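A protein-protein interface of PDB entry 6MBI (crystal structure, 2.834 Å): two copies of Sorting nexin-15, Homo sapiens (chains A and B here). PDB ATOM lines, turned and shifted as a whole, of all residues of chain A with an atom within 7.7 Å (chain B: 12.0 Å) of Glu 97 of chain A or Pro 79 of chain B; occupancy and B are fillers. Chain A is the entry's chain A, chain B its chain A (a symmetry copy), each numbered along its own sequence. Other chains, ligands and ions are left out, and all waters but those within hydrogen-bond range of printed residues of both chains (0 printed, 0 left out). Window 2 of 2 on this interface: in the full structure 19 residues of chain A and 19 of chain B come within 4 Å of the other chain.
OH of Tyr 54 of chain A lies close to O of Pro 79 of chain B, at 3.2 Å. The backbone carbonyl oxygen of Glu 97 of chain A sits close to the backbone carbonyl oxygen of Pro 79 of chain B (3.5 Å).
Phe 78 of chain B touches Tyr 54 of chain A (CZ to CZ, 3.3 Å). Glu 76 of chain B touches His 61 of chain A (CG to CE1, 3.7 Å). Glu 77 of chain B touches His 61 of chain A (O to CE1, 3.7 Å). His 61 of chain A touches Phe 78 of chain B. Gly 101 of chain A touches Pro 79 of chain B (CA to O, 3.96 Å). CD1 of Leu 105 of chain A touches OE2 of Glu 76 of chain B, at 3.8 Å. CD2 of Leu 105 of chain A touches CD1 of Phe 78 of chain B, 3.8 Å away.
Of chain B, only Pro 79 (3.5 Å) comes within 4 Å of Glu 97 of chain A. Pro 79 of chain B touches three residues of chain A. No residue of chain B comes within 4 Å of Ser 93 of chain A. No residue of chain B comes within 4 Å of Val 94 of chain A. No residue of chain B comes within 4 Å of Ile 95 of chain A. No residue of chain B comes within 4 Å of Glu 96 of chain A. No residue of chain B comes within 4 Å of Arg 99 of chain A. No residue of chain B comes within 4 Å of Lys 100 of chain A. Printed residues of chain B within 4 Å of Gly 101 of chain A: Pro 79 (3.96 Å). Of the printed residues of chain B, His 61 of chain A touches Glu 76 (3.7 Å), Glu 77 (3.7 Å) and Phe 78 (3.4 Å). Printed residues of chain A within 4 Å of Glu 77 of chain B: His 61. Printed residues of chain B within 4 Å of Leu 105 of chain A: Glu 76 and Phe 78. Ala 102 of chain A touches none of the printed residues of chain B. The nearest residue of chain B that does not touch Glu 97 of chain A is Phe 78 of chain B (7.3 Å). The nearest residue of chain A that does not touch Pro 79 of chain B is Arg 98 of chain A (4.3 Å).
Hydrophobic or aromatic side chains of chain B within 4 Å of the printed part of chain A: Phe 78. Of the 17 printed residues of chain A, 5 touch a printed residue of chain B. Hydrophobic or aromatic side chains of chain A that line the printed part of chain B: Tyr 54, His 61 and Leu 105. Among the printed residues, 9 pairs touch across the chains. Among the printed residues, no Asp or Glu carboxylate lies within 4 Å of a Lys or Arg side-chain nitrogen of the other chain.
No position is printed for both chains. Of the 9 pairs that touch across the chains among the printed residues, none has its exchanged pair printed and touching as well.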
ATOM      1  N   TYR A  30      -2.696  -1.663   0.297  1.00  0.00           N
ATOM      2  CA  TYR A  30      -3.614  -1.108  -0.685  1.00  0.00           C
ATOM      3  C   TYR A  30      -2.923  -0.054  -1.544  1.00  0.00           C
ATOM      4  O   TYR A  30      -2.186   0.801  -1.035  1.00  0.00           O
ATOM      5  CB  TYR A  30      -4.838  -0.501   0.005  1.00  0.00           C
ATOM      6  CG  TYR A  30      -5.588  -1.465   0.896  1.00  0.00           C
ATOM      7  CD1 TYR A  30      -6.578  -2.291   0.379  1.00  0.00           C
ATOM      8  CD2 TYR A  30      -5.308  -1.548   2.255  1.00  0.00           C
ATOM      9  CE1 TYR A  30      -7.267  -3.175   1.191  1.00  0.00           C
ATOM     10  CE2 TYR A  30      -5.991  -2.426   3.073  1.00  0.00           C
ATOM     11  CZ  TYR A  30      -6.968  -3.237   2.536  1.00  0.00           C
ATOM     12  OH  TYR A  30      -7.650  -4.113   3.349  1.00  0.00           O
ATOM     13  N   TYR A  54      -4.105  -0.253   6.428  1.00  0.00           N
ATOM     14  CA  TYR A  54      -5.339   0.233   7.038  1.00  0.00           C
ATOM     15  C   TYR A  54      -5.093   1.047   8.309  1.00  0.00           C
ATOM     16  O   TYR A  54      -5.944   1.836   8.721  1.00  0.00           O
ATOM     17  CB  TYR A  54      -6.273  -0.940   7.340  1.00  0.00           C
ATOM     18  CG  TYR A  54      -7.733  -0.551   7.399  1.00  0.00           C
ATOM     19  CD1 TYR A  54      -8.392  -0.088   6.265  1.00  0.00           C
ATOM     20  CD2 TYR A  54      -8.455  -0.650   8.581  1.00  0.00           C
ATOM     21  CE1 TYR A  54      -9.725   0.270   6.310  1.00  0.00           C
ATOM     22  CE2 TYR A  54      -9.791  -0.296   8.634  1.00  0.00           C
ATOM     23  CZ  TYR A  54     -10.421   0.162   7.495  1.00  0.00           C
ATOM     24  OH  TYR A  54     -11.750   0.517   7.543  1.00  0.00           O
ATOM     25  N   HIS A  61      -7.923   9.064   8.990  1.00  0.00           N
ATOM     26  CA  HIS A  61      -9.342   9.213   9.290  1.00  0.00           C
ATOM     27  C   HIS A  61      -9.563   9.953  10.598  1.00  0.00           C
ATOM     28  O   HIS A  61     -10.458  10.782  10.696  1.00  0.00           O
ATOM     29  CB  HIS A  61     -10.034   7.853   9.362  1.00  0.00           C
ATOM     30  CG  HIS A  61     -11.353   7.892  10.066  1.00  0.00           C
ATOM     31  ND1 HIS A  61     -12.457   8.528   9.543  1.00  0.00           N
ATOM     32  CD2 HIS A  61     -11.742   7.386  11.261  1.00  0.00           C
ATOM     33  CE1 HIS A  61     -13.472   8.407  10.381  1.00  0.00           C
ATOM     34  NE2 HIS A  61     -13.063   7.717  11.431  1.00  0.00           N
ATOM     35  N   ALA A  92     -11.651 -13.980   3.328  1.00  0.00           N
ATOM     36  CA  ALA A  92     -11.219 -12.678   3.822  1.00  0.00           C
ATOM     37  C   ALA A  92     -11.657 -11.567   2.875  1.00  0.00           C
ATOM     38  O   ALA A  92     -10.827 -10.842   2.328  1.00  0.00           O
ATOM     39  CB  ALA A  92      -9.709 -12.654   4.007  1.00  0.00           C
ATOM     40  N   SER A  93     -12.966 -11.441   2.689  1.00  0.00           N
ATOM     41  CA  SER A  93     -13.522 -10.432   1.795  1.00  0.00           C
ATOM     42  C   SER A  93     -13.772  -9.115   2.524  1.00  0.00           C
ATOM     43  O   SER A  93     -14.460  -8.233   2.013  1.00  0.00           O
ATOM     44  CB  SER A  93     -14.821 -10.936   1.161  1.00  0.00           C
ATOM     45  OG  SER A  93     -15.770 -11.287   2.154  1.00  0.00           O
ATOM     46  N   VAL A  94     -13.210  -8.989   3.723  1.00  0.00           N
ATOM     47  CA  VAL A  94     -13.338  -7.764   4.501  1.00  0.00           C
ATOM     48  C   VAL A  94     -12.378  -6.698   3.983  1.00  0.00           C
ATOM     49  O   VAL A  94     -12.552  -5.505   4.246  1.00  0.00           O
ATOM     50  CB  VAL A  94     -13.072  -8.012   5.997  1.00  0.00           C
ATOM     51  CG1 VAL A  94     -14.103  -8.976   6.564  1.00  0.00           C
ATOM     52  CG2 VAL A  94     -11.664  -8.545   6.208  1.00  0.00           C
ATOM     53  N   ILE A  95     -11.366  -7.136   3.240  1.00  0.00           N
ATOM     54  CA  ILE A  95     -10.398  -6.222   2.645  1.00  0.00           C
ATOM     55  C   ILE A  95     -11.045  -5.415   1.524  1.00  0.00           C
ATOM     56  O   ILE A  95     -10.570  -4.336   1.170  1.00  0.00           O
ATOM     57  CB  ILE A  95      -9.168  -6.977   2.098  1.00  0.00           C
ATOM     58  CG1 ILE A  95      -9.590  -7.996   1.037  1.00  0.00           C
ATOM     59  CG2 ILE A  95      -8.417  -7.664   3.229  1.00  0.00           C
ATOM     60  CD1 ILE A  95      -8.441  -8.801   0.472  1.00  0.00           C
ATOM     61  N   GLU A  96     -12.132  -5.946   0.973  1.00  0.00           N
ATOM     62  CA  GLU A  96     -12.906  -5.241  -0.039  1.00  0.00           C
ATOM     63  C   GLU A  96     -13.665  -4.082   0.596  1.00  0.00           C
ATOM     64  O   GLU A  96     -13.686  -2.970   0.067  1.00  0.00           O
ATOM     65  CB  GLU A  96     -13.878  -6.197  -0.736  1.00  0.00           C
ATOM     66  CG  GLU A  96     -14.804  -5.531  -1.743  1.00  0.00           C
ATOM     67  CD  GLU A  96     -14.082  -5.076  -2.996  1.00  0.00           C
ATOM     68  OE1 GLU A  96     -14.612  -4.190  -3.699  1.00  0.00           O
ATOM     69  OE2 GLU A  96     -12.988  -5.607  -3.282  1.00  0.00           O
ATOM     70  N   GLU A  97     -14.284  -4.356   1.741  1.00  0.00           N
ATOM     71  CA  GLU A  97     -15.023  -3.341   2.479  1.00  0.00           C
ATOM     72  C   GLU A  97     -14.071  -2.288   3.035  1.00  0.00           C
ATOM     73  O   GLU A  97     -14.409  -1.107   3.104  1.00  0.00           O
ATOM     74  CB  GLU A  97     -15.833  -3.979   3.611  1.00  0.00           C
ATOM     75  CG  GLU A  97     -16.637  -5.205   3.194  1.00  0.00           C
ATOM     76  CD  GLU A  97     -17.720  -4.892   2.177  1.00  0.00           C
ATOM     77  OE1 GLU A  97     -18.180  -3.731   2.126  1.00  0.00           O
ATOM     78  OE2 GLU A  97     -18.112  -5.810   1.426  1.00  0.00           O
ATOM     79  N   ARG A  98     -12.881  -2.725   3.436  1.00  0.00           N
ATOM     80  CA  ARG A  98     -11.841  -1.804   3.884  1.00  0.00           C
ATOM     81  C   ARG A  98     -11.378  -0.918   2.733  1.00  0.00           C
ATOM     82  O   ARG A  98     -11.169   0.286   2.902  1.00  0.00           O
ATOM     83  CB  ARG A  98     -10.653  -2.568   4.470  1.00  0.00           C
ATOM     84  CG  ARG A  98     -10.897  -3.134   5.859  1.00  0.00           C
ATOM     85  CD  ARG A  98      -9.602  -3.622   6.488  1.00  0.00           C
ATOM     86  NE  ARG A  98      -9.780  -3.996   7.887  1.00  0.00           N
ATOM     87  CZ  ARG A  98      -8.791  -4.370   8.691  1.00  0.00           C
ATOM     88  NH1 ARG A  98      -7.545  -4.420   8.237  1.00  0.00           N
ATOM     89  NH2 ARG A  98      -9.045  -4.693   9.952  1.00  0.00           N
ATOM     90  N   ARG A  99     -11.221  -1.531   1.563  1.00  0.00           N
ATOM     91  CA  ARG A  99     -10.840  -0.813   0.351  1.00  0.00           C
ATOM     92  C   ARG A  99     -11.854   0.276   0.019  1.00  0.00           C
ATOM     93  O   ARG A  99     -11.495   1.441  -0.177  1.00  0.00           O
ATOM     94  CB  ARG A  99     -10.715  -1.782  -0.827  1.00  0.00           C
ATOM     95  CG  ARG A  99     -10.316  -1.118  -2.133  1.00  0.00           C
ATOM     96  CD  ARG A  99     -10.759  -1.937  -3.335  1.00  0.00           C
ATOM     97  NE  ARG A  99     -12.214  -2.063  -3.400  1.00  0.00           N
ATOM     98  CZ  ARG A  99     -13.023  -1.140  -3.912  1.00  0.00           C
ATOM     99  NH1 ARG A  99     -12.523  -0.016  -4.406  1.00  0.00           N
ATOM    100  NH2 ARG A  99     -14.333  -1.341  -3.928  1.00  0.00           N
ATOM    101  N   LYS A 100     -13.124  -0.115  -0.039  1.00  0.00           N
ATOM    102  CA  LYS A 100     -14.202   0.811  -0.365  1.00  0.00           C
ATOM    103  C   LYS A 100     -14.337   1.896   0.700  1.00  0.00           C
ATOM    104  O   LYS A 100     -14.667   3.040   0.392  1.00  0.00           O
ATOM    105  CB  LYS A 100     -15.521   0.054  -0.526  1.00  0.00           C
ATOM    106  CG  LYS A 100     -16.644   0.878  -1.129  1.00  0.00           C
ATOM    107  CD  LYS A 100     -17.892   0.037  -1.345  1.00  0.00           C
ATOM    108  CE  LYS A 100     -18.987   0.838  -2.026  1.00  0.00           C
ATOM    109  NZ  LYS A 100     -18.564   1.325  -3.370  1.00  0.00           N
ATOM    110  N   GLY A 101     -14.073   1.529   1.952  1.00  0.00           N
ATOM    111  CA  GLY A 101     -14.134   2.471   3.055  1.00  0.00           C
ATOM    112  C   GLY A 101     -13.067   3.544   2.955  1.00  0.00           C
ATOM    113  O   GLY A 101     -13.353   4.736   3.098  1.00  0.00           O
ATOM    114  N   ALA A 102     -11.831   3.120   2.711  1.00  0.00           N
ATOM    115  CA  ALA A 102     -10.725   4.053   2.532  1.00  0.00           C
ATOM    116  C   ALA A 102     -10.953   4.926   1.300  1.00  0.00           C
ATOM    117  O   ALA A 102     -10.626   6.117   1.295  1.00  0.00           O
ATOM    118  CB  ALA A 102      -9.410   3.301   2.416  1.00  0.00           C
ATOM    119  N   GLU A 103     -11.523   4.323   0.261  1.00  0.00           N
ATOM    120  CA  GLU A 103     -11.829   5.038  -0.973  1.00  0.00           C
ATOM    121  C   GLU A 103     -12.849   6.144  -0.721  1.00  0.00           C
ATOM    122  O   GLU A 103     -12.688   7.272  -1.192  1.00  0.00           O
ATOM    123  CB  GLU A 103     -12.348   4.069  -2.037  1.00  0.00           C
ATOM    124  CG  GLU A 103     -12.330   4.625  -3.449  1.00  0.00           C
ATOM    125  CD  GLU A 103     -12.729   3.592  -4.485  1.00  0.00           C
ATOM    126  OE1 GLU A 103     -13.890   3.131  -4.446  1.00  0.00           O
ATOM    127  OE2 GLU A 103     -11.882   3.236  -5.332  1.00  0.00           O
ATOM    128  N   ASP A 104     -13.896   5.813   0.030  1.00  0.00           N
ATOM    129  CA  ASP A 104     -14.915   6.790   0.400  1.00  0.00           C
ATOM    130  C   ASP A 104     -14.315   7.895   1.260  1.00  0.00           C
ATOM    131  O   ASP A 104     -14.653   9.070   1.103  1.00  0.00           O
ATOM    132  CB  ASP A 104     -16.068   6.115   1.145  1.00  0.00           C
ATOM    133  CG  ASP A 104     -16.875   5.191   0.255  1.00  0.00           C
ATOM    134  OD1 ASP A 104     -16.908   5.424  -0.971  1.00  0.00           O
ATOM    135  OD2 ASP A 104     -17.481   4.233   0.782  1.00  0.00           O
ATOM    136  N   LEU A 105     -13.424   7.506   2.168  1.00  0.00           N
ATOM    137  CA  LEU A 105     -12.746   8.460   3.037  1.00  0.00           C
ATOM    138  C   LEU A 105     -11.955   9.478   2.224  1.00  0.00           C
ATOM    139  O   LEU A 105     -12.035  10.682   2.469  1.00  0.00           O
ATOM    140  CB  LEU A 105     -11.817   7.734   4.012  1.00  0.00           C
ATOM    141  CG  LEU A 105     -10.991   8.623   4.942  1.00  0.00           C
ATOM    142  CD1 LEU A 105     -11.895   9.440   5.849  1.00  0.00           C
ATOM    143  CD2 LEU A 105     -10.019   7.783   5.756  1.00  0.00           C
ATOM    144  N   LEU B  75     -21.727  13.074   6.582  1.00  0.00           N
ATOM    145  CA  LEU B  75     -21.155  12.260   7.651  1.00  0.00           C
ATOM    146  C   LEU B  75     -19.631  12.199   7.559  1.00  0.00           C
ATOM    147  O   LEU B  75     -18.976  13.204   7.286  1.00  0.00           O
ATOM    148  CB  LEU B  75     -21.734  10.842   7.624  1.00  0.00           C
ATOM    149  CG  LEU B  75     -23.193  10.632   8.043  1.00  0.00           C
ATOM    150  CD1 LEU B  75     -24.153  10.983   6.916  1.00  0.00           C
ATOM    151  CD2 LEU B  75     -23.405   9.194   8.488  1.00  0.00           C
ATOM    152  N   GLU B  76     -19.077  11.013   7.789  1.00  0.00           N
ATOM    153  CA  GLU B  76     -17.634  10.805   7.741  1.00  0.00           C
ATOM    154  C   GLU B  76     -17.317   9.334   7.485  1.00  0.00           C
ATOM    155  O   GLU B  76     -16.932   8.959   6.374  1.00  0.00           O
ATOM    156  CB  GLU B  76     -16.980  11.275   9.043  1.00  0.00           C
ATOM    157  CG  GLU B  76     -15.461  11.184   9.055  1.00  0.00           C
ATOM    158  CD  GLU B  76     -14.798  12.258   8.212  1.00  0.00           C
ATOM    159  OE1 GLU B  76     -15.497  13.196   7.778  1.00  0.00           O
ATOM    160  OE2 GLU B  76     -13.572  12.162   7.987  1.00  0.00           O
ATOM    161  N   GLU B  77     -17.467   8.521   8.532  1.00  0.00           N
ATOM    162  CA  GLU B  77     -17.398   7.058   8.460  1.00  0.00           C
ATOM    163  C   GLU B  77     -16.009   6.491   8.154  1.00  0.00           C
ATOM    164  O   GLU B  77     -15.219   7.093   7.426  1.00  0.00           O
ATOM    165  CB  GLU B  77     -18.391   6.535   7.418  1.00  0.00           C
ATOM    166  CG  GLU B  77     -19.826   6.968   7.652  1.00  0.00           C
ATOM    167  CD  GLU B  77     -20.718   6.677   6.462  1.00  0.00           C
ATOM    168  OE1 GLU B  77     -20.196   6.209   5.428  1.00  0.00           O
ATOM    169  OE2 GLU B  77     -21.941   6.919   6.560  1.00  0.00           O
ATOM    170  N   PHE B  78     -15.736   5.319   8.723  1.00  0.00           N
ATOM    171  CA  PHE B  78     -14.513   4.565   8.457  1.00  0.00           C
ATOM    172  C   PHE B  78     -14.618   3.161   9.040  1.00  0.00           C
ATOM    173  O   PHE B  78     -14.456   2.966  10.245  1.00  0.00           O
ATOM    174  CB  PHE B  78     -13.288   5.277   9.037  1.00  0.00           C
ATOM    175  CG  PHE B  78     -11.988   4.565   8.775  1.00  0.00           C
ATOM    176  CD1 PHE B  78     -11.355   4.681   7.548  1.00  0.00           C
ATOM    177  CD2 PHE B  78     -11.398   3.789   9.758  1.00  0.00           C
ATOM    178  CE1 PHE B  78     -10.160   4.031   7.305  1.00  0.00           C
ATOM    179  CE2 PHE B  78     -10.202   3.137   9.521  1.00  0.00           C
ATOM    180  CZ  PHE B  78      -9.582   3.259   8.293  1.00  0.00           C
ATOM    181  N   PRO B  79     -14.890   2.183   8.182  1.00  0.00           N
ATOM    182  CA  PRO B  79     -15.006   0.795   8.617  1.00  0.00           C
ATOM    183  C   PRO B  79     -14.795  -0.160   7.449  1.00  0.00           C
ATOM    184  O   PRO B  79     -14.672   0.267   6.302  1.00  0.00           O
ATOM    185  CB  PRO B  79     -16.362   0.555   9.264  1.00  0.00           C
